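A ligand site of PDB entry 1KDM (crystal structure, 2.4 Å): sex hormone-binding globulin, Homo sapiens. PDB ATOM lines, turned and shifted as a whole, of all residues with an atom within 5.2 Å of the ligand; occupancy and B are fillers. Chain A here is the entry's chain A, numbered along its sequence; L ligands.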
ATOM      1  N   THR A  29     -20.005   3.892 -13.177  1.00  0.00           N
ATOM      2  CA  THR A  29     -18.784   3.220 -13.588  1.00  0.00           C
ATOM      3  C   THR A  29     -19.141   2.091 -14.544  1.00  0.00           C
ATOM      4  O   THR A  29     -19.046   0.910 -14.211  1.00  0.00           O
ATOM      5  CB  THR A  29     -18.078   2.708 -12.320  1.00  0.00           C
ATOM      6  OG1 THR A  29     -18.989   1.812 -11.668  1.00  0.00           O
ATOM      7  CG2 THR A  29     -17.699   3.768 -11.296  1.00  0.00           C
ATOM      8  N   SER A  30     -19.773   2.432 -15.639  1.00  0.00           N
ATOM      9  CA  SER A  30     -20.156   1.539 -16.722  1.00  0.00           C
ATOM     10  C   SER A  30     -20.210   2.324 -18.021  1.00  0.00           C
ATOM     11  O   SER A  30     -20.399   3.533 -18.080  1.00  0.00           O
ATOM     12  CB  SER A  30     -21.522   0.881 -16.514  1.00  0.00           C
ATOM     13  OG  SER A  30     -22.533   1.887 -16.545  1.00  0.00           O
ATOM     14  N   SER A  31     -20.092   1.626 -19.114  1.00  0.00           N
ATOM     15  CA  SER A  31     -20.164   2.122 -20.472  1.00  0.00           C
ATOM     16  C   SER A  31     -21.047   1.172 -21.255  1.00  0.00           C
ATOM     17  O   SER A  31     -21.135   0.004 -20.876  1.00  0.00           O
ATOM     18  CB  SER A  31     -18.739   2.090 -21.064  1.00  0.00           C
ATOM     19  OG  SER A  31     -17.927   2.911 -20.200  1.00  0.00           O
ATOM     20  N   PHE A  45     -12.445  -0.740 -27.338  1.00  0.00           N
ATOM     21  CA  PHE A  45     -12.105   0.439 -26.561  1.00  0.00           C
ATOM     22  C   PHE A  45     -11.002   0.119 -25.556  1.00  0.00           C
ATOM     23  O   PHE A  45     -10.734  -1.021 -25.236  1.00  0.00           O
ATOM     24  CB  PHE A  45     -13.280   1.131 -25.895  1.00  0.00           C
ATOM     25  CG  PHE A  45     -13.808   0.521 -24.639  1.00  0.00           C
ATOM     26  CD1 PHE A  45     -13.285   0.902 -23.405  1.00  0.00           C
ATOM     27  CD2 PHE A  45     -14.792  -0.467 -24.704  1.00  0.00           C
ATOM     28  CE1 PHE A  45     -13.852   0.368 -22.264  1.00  0.00           C
ATOM     29  CE2 PHE A  45     -15.293  -1.045 -23.539  1.00  0.00           C
ATOM     30  CZ  PHE A  45     -14.833  -0.613 -22.308  1.00  0.00           C
ATOM     31  N   GLY A  47      -9.174   1.879 -21.888  1.00  0.00           N
ATOM     32  CA  GLY A  47      -9.302   2.849 -20.792  1.00  0.00           C
ATOM     33  C   GLY A  47      -7.974   2.814 -20.018  1.00  0.00           C
ATOM     34  O   GLY A  47      -7.327   1.726 -20.019  1.00  0.00           O
ATOM     35  N   ASP A  48      -7.571   3.880 -19.368  1.00  0.00           N
ATOM     36  CA  ASP A  48      -6.400   3.893 -18.509  1.00  0.00           C
ATOM     37  C   ASP A  48      -6.429   5.072 -17.525  1.00  0.00           C
ATOM     38  O   ASP A  48      -7.290   5.976 -17.518  1.00  0.00           O
ATOM     39  CB  ASP A  48      -5.113   3.876 -19.316  1.00  0.00           C
ATOM     40  CG  ASP A  48      -4.637   5.144 -19.971  1.00  0.00           C
ATOM     41  OD1 ASP A  48      -5.184   6.270 -19.871  1.00  0.00           O
ATOM     42  OD2 ASP A  48      -3.671   5.163 -20.754  1.00  0.00           O
ATOM     43  N   THR A  49      -5.634   4.932 -16.457  1.00  0.00           N
ATOM     44  CA  THR A  49      -5.194   6.063 -15.670  1.00  0.00           C
ATOM     45  C   THR A  49      -3.677   6.278 -15.892  1.00  0.00           C
ATOM     46  O   THR A  49      -3.177   7.380 -15.678  1.00  0.00           O
ATOM     47  CB  THR A  49      -5.487   6.150 -14.189  1.00  0.00           C
ATOM     48  OG1 THR A  49      -4.654   5.229 -13.469  1.00  0.00           O
ATOM     49  CG2 THR A  49      -6.959   6.027 -13.830  1.00  0.00           C
ATOM     50  N   ASP A  54      -1.902   0.873 -15.431  1.00  0.00           N
ATOM     51  CA  ASP A  54      -3.295   0.952 -14.972  1.00  0.00           C
ATOM     52  C   ASP A  54      -4.162   1.114 -16.214  1.00  0.00           C
ATOM     53  O   ASP A  54      -4.474   2.219 -16.632  1.00  0.00           O
ATOM     54  CB  ASP A  54      -3.449   2.019 -13.896  1.00  0.00           C
ATOM     55  CG  ASP A  54      -4.787   1.959 -13.178  1.00  0.00           C
ATOM     56  OD1 ASP A  54      -5.273   0.888 -12.716  1.00  0.00           O
ATOM     57  OD2 ASP A  54      -5.458   3.022 -13.098  1.00  0.00           O
ATOM     58  N   TRP A  55      -4.414   0.016 -16.935  1.00  0.00           N
ATOM     59  CA  TRP A  55      -5.029   0.032 -18.247  1.00  0.00           C
ATOM     60  C   TRP A  55      -5.881  -1.198 -18.547  1.00  0.00           C
ATOM     61  O   TRP A  55      -5.843  -2.267 -17.929  1.00  0.00           O
ATOM     62  CB  TRP A  55      -3.935   0.287 -19.287  1.00  0.00           C
ATOM     63  CG  TRP A  55      -2.939  -0.833 -19.461  1.00  0.00           C
ATOM     64  CD1 TRP A  55      -1.689  -0.953 -18.930  1.00  0.00           C
ATOM     65  CD2 TRP A  55      -3.140  -2.003 -20.275  1.00  0.00           C
ATOM     66  NE1 TRP A  55      -1.093  -2.135 -19.356  1.00  0.00           N
ATOM     67  CE2 TRP A  55      -1.974  -2.787 -20.169  1.00  0.00           C
ATOM     68  CE3 TRP A  55      -4.233  -2.470 -21.006  1.00  0.00           C
ATOM     69  CZ2 TRP A  55      -1.848  -4.048 -20.793  1.00  0.00           C
ATOM     70  CZ3 TRP A  55      -4.093  -3.698 -21.640  1.00  0.00           C
ATOM     71  CH2 TRP A  55      -2.921  -4.461 -21.555  1.00  0.00           C
ATOM     72  N   PHE A  56      -6.848  -1.008 -19.448  1.00  0.00           N
ATOM     73  CA  PHE A  56      -7.877  -1.994 -19.766  1.00  0.00           C
ATOM     74  C   PHE A  56      -8.140  -1.856 -21.260  1.00  0.00           C
ATOM     75  O   PHE A  56      -8.166  -0.786 -21.829  1.00  0.00           O
ATOM     76  CB  PHE A  56      -9.152  -1.742 -18.991  1.00  0.00           C
ATOM     77  CG  PHE A  56     -10.388  -2.503 -19.382  1.00  0.00           C
ATOM     78  CD1 PHE A  56     -10.800  -3.579 -18.615  1.00  0.00           C
ATOM     79  CD2 PHE A  56     -11.170  -2.135 -20.494  1.00  0.00           C
ATOM     80  CE1 PHE A  56     -11.927  -4.303 -18.922  1.00  0.00           C
ATOM     81  CE2 PHE A  56     -12.319  -2.852 -20.782  1.00  0.00           C
ATOM     82  CZ  PHE A  56     -12.657  -3.988 -20.082  1.00  0.00           C
ATOM     83  N   LEU A  69      -6.112  -6.558 -19.248  1.00  0.00           N
ATOM     84  CA  LEU A  69      -6.115  -5.593 -18.134  1.00  0.00           C
ATOM     85  C   LEU A  69      -4.835  -5.746 -17.350  1.00  0.00           C
ATOM     86  O   LEU A  69      -4.431  -6.850 -16.976  1.00  0.00           O
ATOM     87  CB  LEU A  69      -7.324  -6.039 -17.349  1.00  0.00           C
ATOM     88  CG  LEU A  69      -7.839  -5.607 -16.015  1.00  0.00           C
ATOM     89  CD1 LEU A  69      -9.282  -6.087 -15.935  1.00  0.00           C
ATOM     90  CD2 LEU A  69      -7.037  -6.228 -14.873  1.00  0.00           C
ATOM     91  N   ASN A  71      -3.407  -3.582 -13.841  1.00  0.00           N
ATOM     92  CA  ASN A  71      -3.547  -2.578 -12.801  1.00  0.00           C
ATOM     93  C   ASN A  71      -2.874  -3.197 -11.569  1.00  0.00           C
ATOM     94  O   ASN A  71      -2.274  -4.281 -11.649  1.00  0.00           O
ATOM     95  CB  ASN A  71      -5.003  -2.196 -12.553  1.00  0.00           C
ATOM     96  CG  ASN A  71      -5.978  -3.194 -12.001  1.00  0.00           C
ATOM     97  OD1 ASN A  71      -5.555  -4.235 -11.474  1.00  0.00           O
ATOM     98  ND2 ASN A  71      -7.299  -2.925 -12.097  1.00  0.00           N
ATOM     99  N   TRP A  73      -4.014  -4.753  -8.886  1.00  0.00           N
ATOM    100  CA  TRP A  73      -4.595  -5.975  -8.348  1.00  0.00           C
ATOM    101  C   TRP A  73      -4.613  -7.162  -9.306  1.00  0.00           C
ATOM    102  O   TRP A  73      -4.732  -8.293  -8.834  1.00  0.00           O
ATOM    103  CB  TRP A  73      -6.047  -5.681  -7.965  1.00  0.00           C
ATOM    104  CG  TRP A  73      -6.195  -4.629  -6.903  1.00  0.00           C
ATOM    105  CD1 TRP A  73      -6.091  -4.808  -5.551  1.00  0.00           C
ATOM    106  CD2 TRP A  73      -6.384  -3.229  -7.127  1.00  0.00           C
ATOM    107  NE1 TRP A  73      -6.263  -3.592  -4.929  1.00  0.00           N
ATOM    108  CE2 TRP A  73      -6.435  -2.610  -5.866  1.00  0.00           C
ATOM    109  CE3 TRP A  73      -6.593  -2.450  -8.275  1.00  0.00           C
ATOM    110  CZ2 TRP A  73      -6.720  -1.252  -5.708  1.00  0.00           C
ATOM    111  CZ3 TRP A  73      -6.828  -1.100  -8.125  1.00  0.00           C
ATOM    112  CH2 TRP A  73      -6.885  -0.503  -6.844  1.00  0.00           C
ATOM    113  N   VAL A  94     -20.117  -2.814 -20.361  1.00  0.00           N
ATOM    114  CA  VAL A  94     -18.987  -3.071 -19.474  1.00  0.00           C
ATOM    115  C   VAL A  94     -19.281  -2.346 -18.153  1.00  0.00           C
ATOM    116  O   VAL A  94     -19.595  -1.142 -18.201  1.00  0.00           O
ATOM    117  CB  VAL A  94     -17.607  -2.725 -20.056  1.00  0.00           C
ATOM    118  CG1 VAL A  94     -16.486  -3.189 -19.112  1.00  0.00           C
ATOM    119  CG2 VAL A  94     -17.345  -3.386 -21.410  1.00  0.00           C
ATOM    120  N   LYS A  95     -19.319  -3.081 -17.038  1.00  0.00           N
ATOM    121  CA  LYS A  95     -19.679  -2.399 -15.786  1.00  0.00           C
ATOM    122  C   LYS A  95     -18.669  -2.765 -14.701  1.00  0.00           C
ATOM    123  O   LYS A  95     -18.429  -3.951 -14.496  1.00  0.00           O
ATOM    124  CB  LYS A  95     -21.009  -2.793 -15.164  1.00  0.00           C
ATOM    125  CG  LYS A  95     -22.209  -3.176 -16.027  1.00  0.00           C
ATOM    126  CD  LYS A  95     -23.463  -3.240 -15.136  1.00  0.00           C
ATOM    127  CE  LYS A  95     -24.709  -3.467 -15.979  1.00  0.00           C
ATOM    128  NZ  LYS A  95     -24.525  -2.832 -17.322  1.00  0.00           N
ATOM    129  N   MET A  96     -18.366  -1.794 -13.836  1.00  0.00           N
ATOM    130  CA  MET A  96     -17.613  -2.110 -12.641  1.00  0.00           C
ATOM    131  C   MET A  96     -18.545  -2.052 -11.439  1.00  0.00           C
ATOM    132  O   MET A  96     -19.382  -1.169 -11.262  1.00  0.00           O
ATOM    133  CB  MET A  96     -16.381  -1.212 -12.538  1.00  0.00           C
ATOM    134  CG  MET A  96     -15.554  -1.628 -11.320  1.00  0.00           C
ATOM    135  SD  MET A  96     -14.318  -0.382 -11.006  1.00  0.00           S
ATOM    136  CE  MET A  96     -14.070  -0.384  -9.238  1.00  0.00           C
ATOM    137  N   VAL A 101     -15.460  -6.574 -12.612  1.00  0.00           N
ATOM    138  CA  VAL A 101     -15.755  -5.941 -13.901  1.00  0.00           C
ATOM    139  C   VAL A 101     -16.651  -6.926 -14.631  1.00  0.00           C
ATOM    140  O   VAL A 101     -16.275  -8.109 -14.699  1.00  0.00           O
ATOM    141  CB  VAL A 101     -14.537  -5.672 -14.802  1.00  0.00           C
ATOM    142  CG1 VAL A 101     -14.986  -5.393 -16.219  1.00  0.00           C
ATOM    143  CG2 VAL A 101     -13.743  -4.506 -14.244  1.00  0.00           C
ATOM    144  N   SER A 117     -10.311  -4.893  -8.998  1.00  0.00           N
ATOM    145  CA  SER A 117     -10.055  -3.457  -8.817  1.00  0.00           C
ATOM    146  C   SER A 117     -10.526  -2.966  -7.458  1.00  0.00           C
ATOM    147  O   SER A 117     -11.496  -3.531  -6.991  1.00  0.00           O
ATOM    148  CB  SER A 117     -10.744  -2.578  -9.875  1.00  0.00           C
ATOM    149  OG  SER A 117     -10.301  -1.244  -9.820  1.00  0.00           O
ATOM    150  N   LEU A 120     -12.677   3.178  -7.511  1.00  0.00           N
ATOM    151  CA  LEU A 120     -12.109   4.157  -8.424  1.00  0.00           C
ATOM    152  C   LEU A 120     -11.809   5.430  -7.640  1.00  0.00           C
ATOM    153  O   LEU A 120     -10.677   5.719  -7.262  1.00  0.00           O
ATOM    154  CB  LEU A 120     -13.123   4.459  -9.528  1.00  0.00           C
ATOM    155  CG  LEU A 120     -12.854   3.931 -10.928  1.00  0.00           C
ATOM    156  CD1 LEU A 120     -11.984   2.690 -10.946  1.00  0.00           C
ATOM    157  CD2 LEU A 120     -14.150   3.671 -11.672  1.00  0.00           C
ATOM    158  N   LYS A 123      -8.530   6.430  -6.057  1.00  0.00           N
ATOM    159  CA  LYS A 123      -7.532   5.945  -6.982  1.00  0.00           C
ATOM    160  C   LYS A 123      -6.346   6.906  -7.143  1.00  0.00           C
ATOM    161  O   LYS A 123      -6.281   8.132  -7.098  1.00  0.00           O
ATOM    162  CB  LYS A 123      -8.010   5.480  -8.352  1.00  0.00           C
ATOM    163  CG  LYS A 123      -7.005   4.831  -9.294  1.00  0.00           C
ATOM    164  CD  LYS A 123      -7.705   4.033 -10.388  1.00  0.00           C
ATOM    165  CE  LYS A 123      -7.005   2.722 -10.656  1.00  0.00           C
ATOM    166  NZ  LYS A 123      -7.964   1.576 -10.658  1.00  0.00           N
ATOM    167  N   MET A 128      -8.902   9.508 -15.758  1.00  0.00           N
ATOM    168  CA  MET A 128      -8.998   8.304 -16.562  1.00  0.00           C
ATOM    169  C   MET A 128      -9.279   8.758 -17.991  1.00  0.00           C
ATOM    170  O   MET A 128     -10.029   9.684 -18.354  1.00  0.00           O
ATOM    171  CB  MET A 128     -10.098   7.434 -15.945  1.00  0.00           C
ATOM    172  CG  MET A 128     -10.631   6.307 -16.849  1.00  0.00           C
ATOM    173  SD  MET A 128     -11.492   5.064 -15.870  1.00  0.00           S
ATOM    174  CE  MET A 128     -10.257   4.583 -14.669  1.00  0.00           C
ATOM    175  N   ILE A 130     -10.432   7.352 -21.870  1.00  0.00           N
ATOM    176  CA  ILE A 130     -11.153   6.349 -22.644  1.00  0.00           C
ATOM    177  C   ILE A 130     -10.860   6.598 -24.128  1.00  0.00           C
ATOM    178  O   ILE A 130     -11.258   7.681 -24.604  1.00  0.00           O
ATOM    179  CB  ILE A 130     -12.696   6.405 -22.479  1.00  0.00           C
ATOM    180  CG1 ILE A 130     -12.992   6.092 -21.014  1.00  0.00           C
ATOM    181  CG2 ILE A 130     -13.451   5.379 -23.341  1.00  0.00           C
ATOM    182  CD1 ILE A 130     -12.745   4.623 -20.672  1.00  0.00           C
ATOM    183  N   LEU A 160     -18.773   5.710 -19.256  1.00  0.00           N
ATOM    184  CA  LEU A 160     -18.606   6.097 -17.850  1.00  0.00           C
ATOM    185  C   LEU A 160     -19.602   7.188 -17.478  1.00  0.00           C
ATOM    186  O   LEU A 160     -20.809   7.114 -17.775  1.00  0.00           O
ATOM    187  CB  LEU A 160     -17.159   6.537 -17.691  1.00  0.00           C
ATOM    188  CG  LEU A 160     -16.068   5.476 -17.482  1.00  0.00           C
ATOM    189  CD1 LEU A 160     -14.677   6.085 -17.395  1.00  0.00           C
ATOM    190  CD2 LEU A 160     -16.329   4.696 -16.198  1.00  0.00           C
HETATM  191  C1  LIG L   1     -14.852   0.256 -15.665  1.00  0.00           C
HETATM  192  C2  LIG L   1     -16.246   0.203 -16.299  1.00  0.00           C
HETATM  193  C3  LIG L   1     -16.256   0.821 -17.694  1.00  0.00           C
HETATM  194  O1  LIG L   1     -17.108   1.691 -17.857  1.00  0.00           O
HETATM  195  C4  LIG L   1     -14.981   0.972 -18.504  1.00  0.00           C
HETATM  196  C5  LIG L   1     -13.718   1.231 -17.662  1.00  0.00           C
HETATM  197  C6  LIG L   1     -12.448   1.194 -18.574  1.00  0.00           C
HETATM  198  C7  LIG L   1     -11.226   1.615 -17.725  1.00  0.00           C
HETATM  199  C8  LIG L   1     -11.055   0.589 -16.579  1.00  0.00           C
HETATM  200  C9  LIG L   1     -12.341   0.440 -15.722  1.00  0.00           C
HETATM  201  C10 LIG L   1     -13.607   0.151 -16.546  1.00  0.00           C
HETATM  202  C11 LIG L   1     -12.114  -0.553 -14.559  1.00  0.00           C
HETATM  203  C12 LIG L   1     -10.891  -0.139 -13.722  1.00  0.00           C
HETATM  204  C13 LIG L   1      -9.606  -0.073 -14.538  1.00  0.00           C
HETATM  205  C14 LIG L   1      -9.871   0.873 -15.716  1.00  0.00           C
HETATM  206  C15 LIG L   1      -8.497   1.193 -16.332  1.00  0.00           C
HETATM  207  C16 LIG L   1      -7.519   0.990 -15.158  1.00  0.00           C
HETATM  208  C17 LIG L   1      -8.392   0.590 -13.950  1.00  0.00           C
HETATM  209  O2  LIG L   1      -7.492  -0.171 -13.090  1.00  0.00           O
HETATM  210  C18 LIG L   1      -9.335  -1.503 -15.068  1.00  0.00           C
HETATM  211  C19 LIG L   1     -13.454  -1.268 -17.139  1.00  0.00           C
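The side-chain amide nitrogen (ND2) of Asn 71 is in hydrogen-bond range of an oxygen (O2) of the ligand (2.9 Å).
The backbone NH (N) of Ser 31 sits at hydrogen-bond distance from an oxygen (O1) of the ligand, 3.2 Å away.
O2 of the ligand is in hydrogen-bond range of OD1 of Asp 54 (2.5 Å).
OG of Ser 31 sits at hydrogen-bond distance from O1 of the ligand (2.8 Å).
The side-chain amino group (NZ) of Lys 123 lies within hydrogen-bond range of an oxygen (O2) of the ligand.
Merely in contact with the ligand: Thr 29 (3.6 Å), Ser 30 (3.2 Å), Phe 45 (3.97 Å), Gly 47 (3.8 Å), Trp 55 (3.7 Å), Phe 56 (3.8 Å), Val 94 (3.8 Å), Met 96 (3.8 Å), Met 128 (3.9 Å) and Leu 160 (3.5 Å).
Hydrophobic or aromatic side chains within 4 Å of the ligand: Phe 45, Phe 56, Met 96, Met 128 and Leu 160.
The nearest printed residue that does not touch the ligand is Ile 130 (4.03 Å).
The side-chain amino group (NZ) of Lys 123 lies within salt-bridge range of the side-chain carboxylate (OD1) of Asp 54 (3.5 Å).
N of Thr 49 sits at hydrogen-bond distance from O of Asp 54, 3.0 Å away.
The backbone NH of Ser 31 sits at hydrogen-bond distance from the backbone carbonyl oxygen of Val 94 (3.0 Å).
OG of Ser 31 lies within hydrogen-bond range of N of Leu 160 (3.1 Å).
N of Phe 56 lies within hydrogen-bond range of O of Gly 47 (2.8 Å).
The side-chain amide oxygen (OD1) of Asn 71 sits at hydrogen-bond distance from the backbone NH (N) of Trp 73, at 3.1 Å.
O of Ser 30 is in hydrogen-bond range of N of Leu 160, 3.0 Å away.
The backbone NH of Met 96 sits at hydrogen-bond distance from the backbone carbonyl oxygen of Thr 29, at 2.8 Å.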
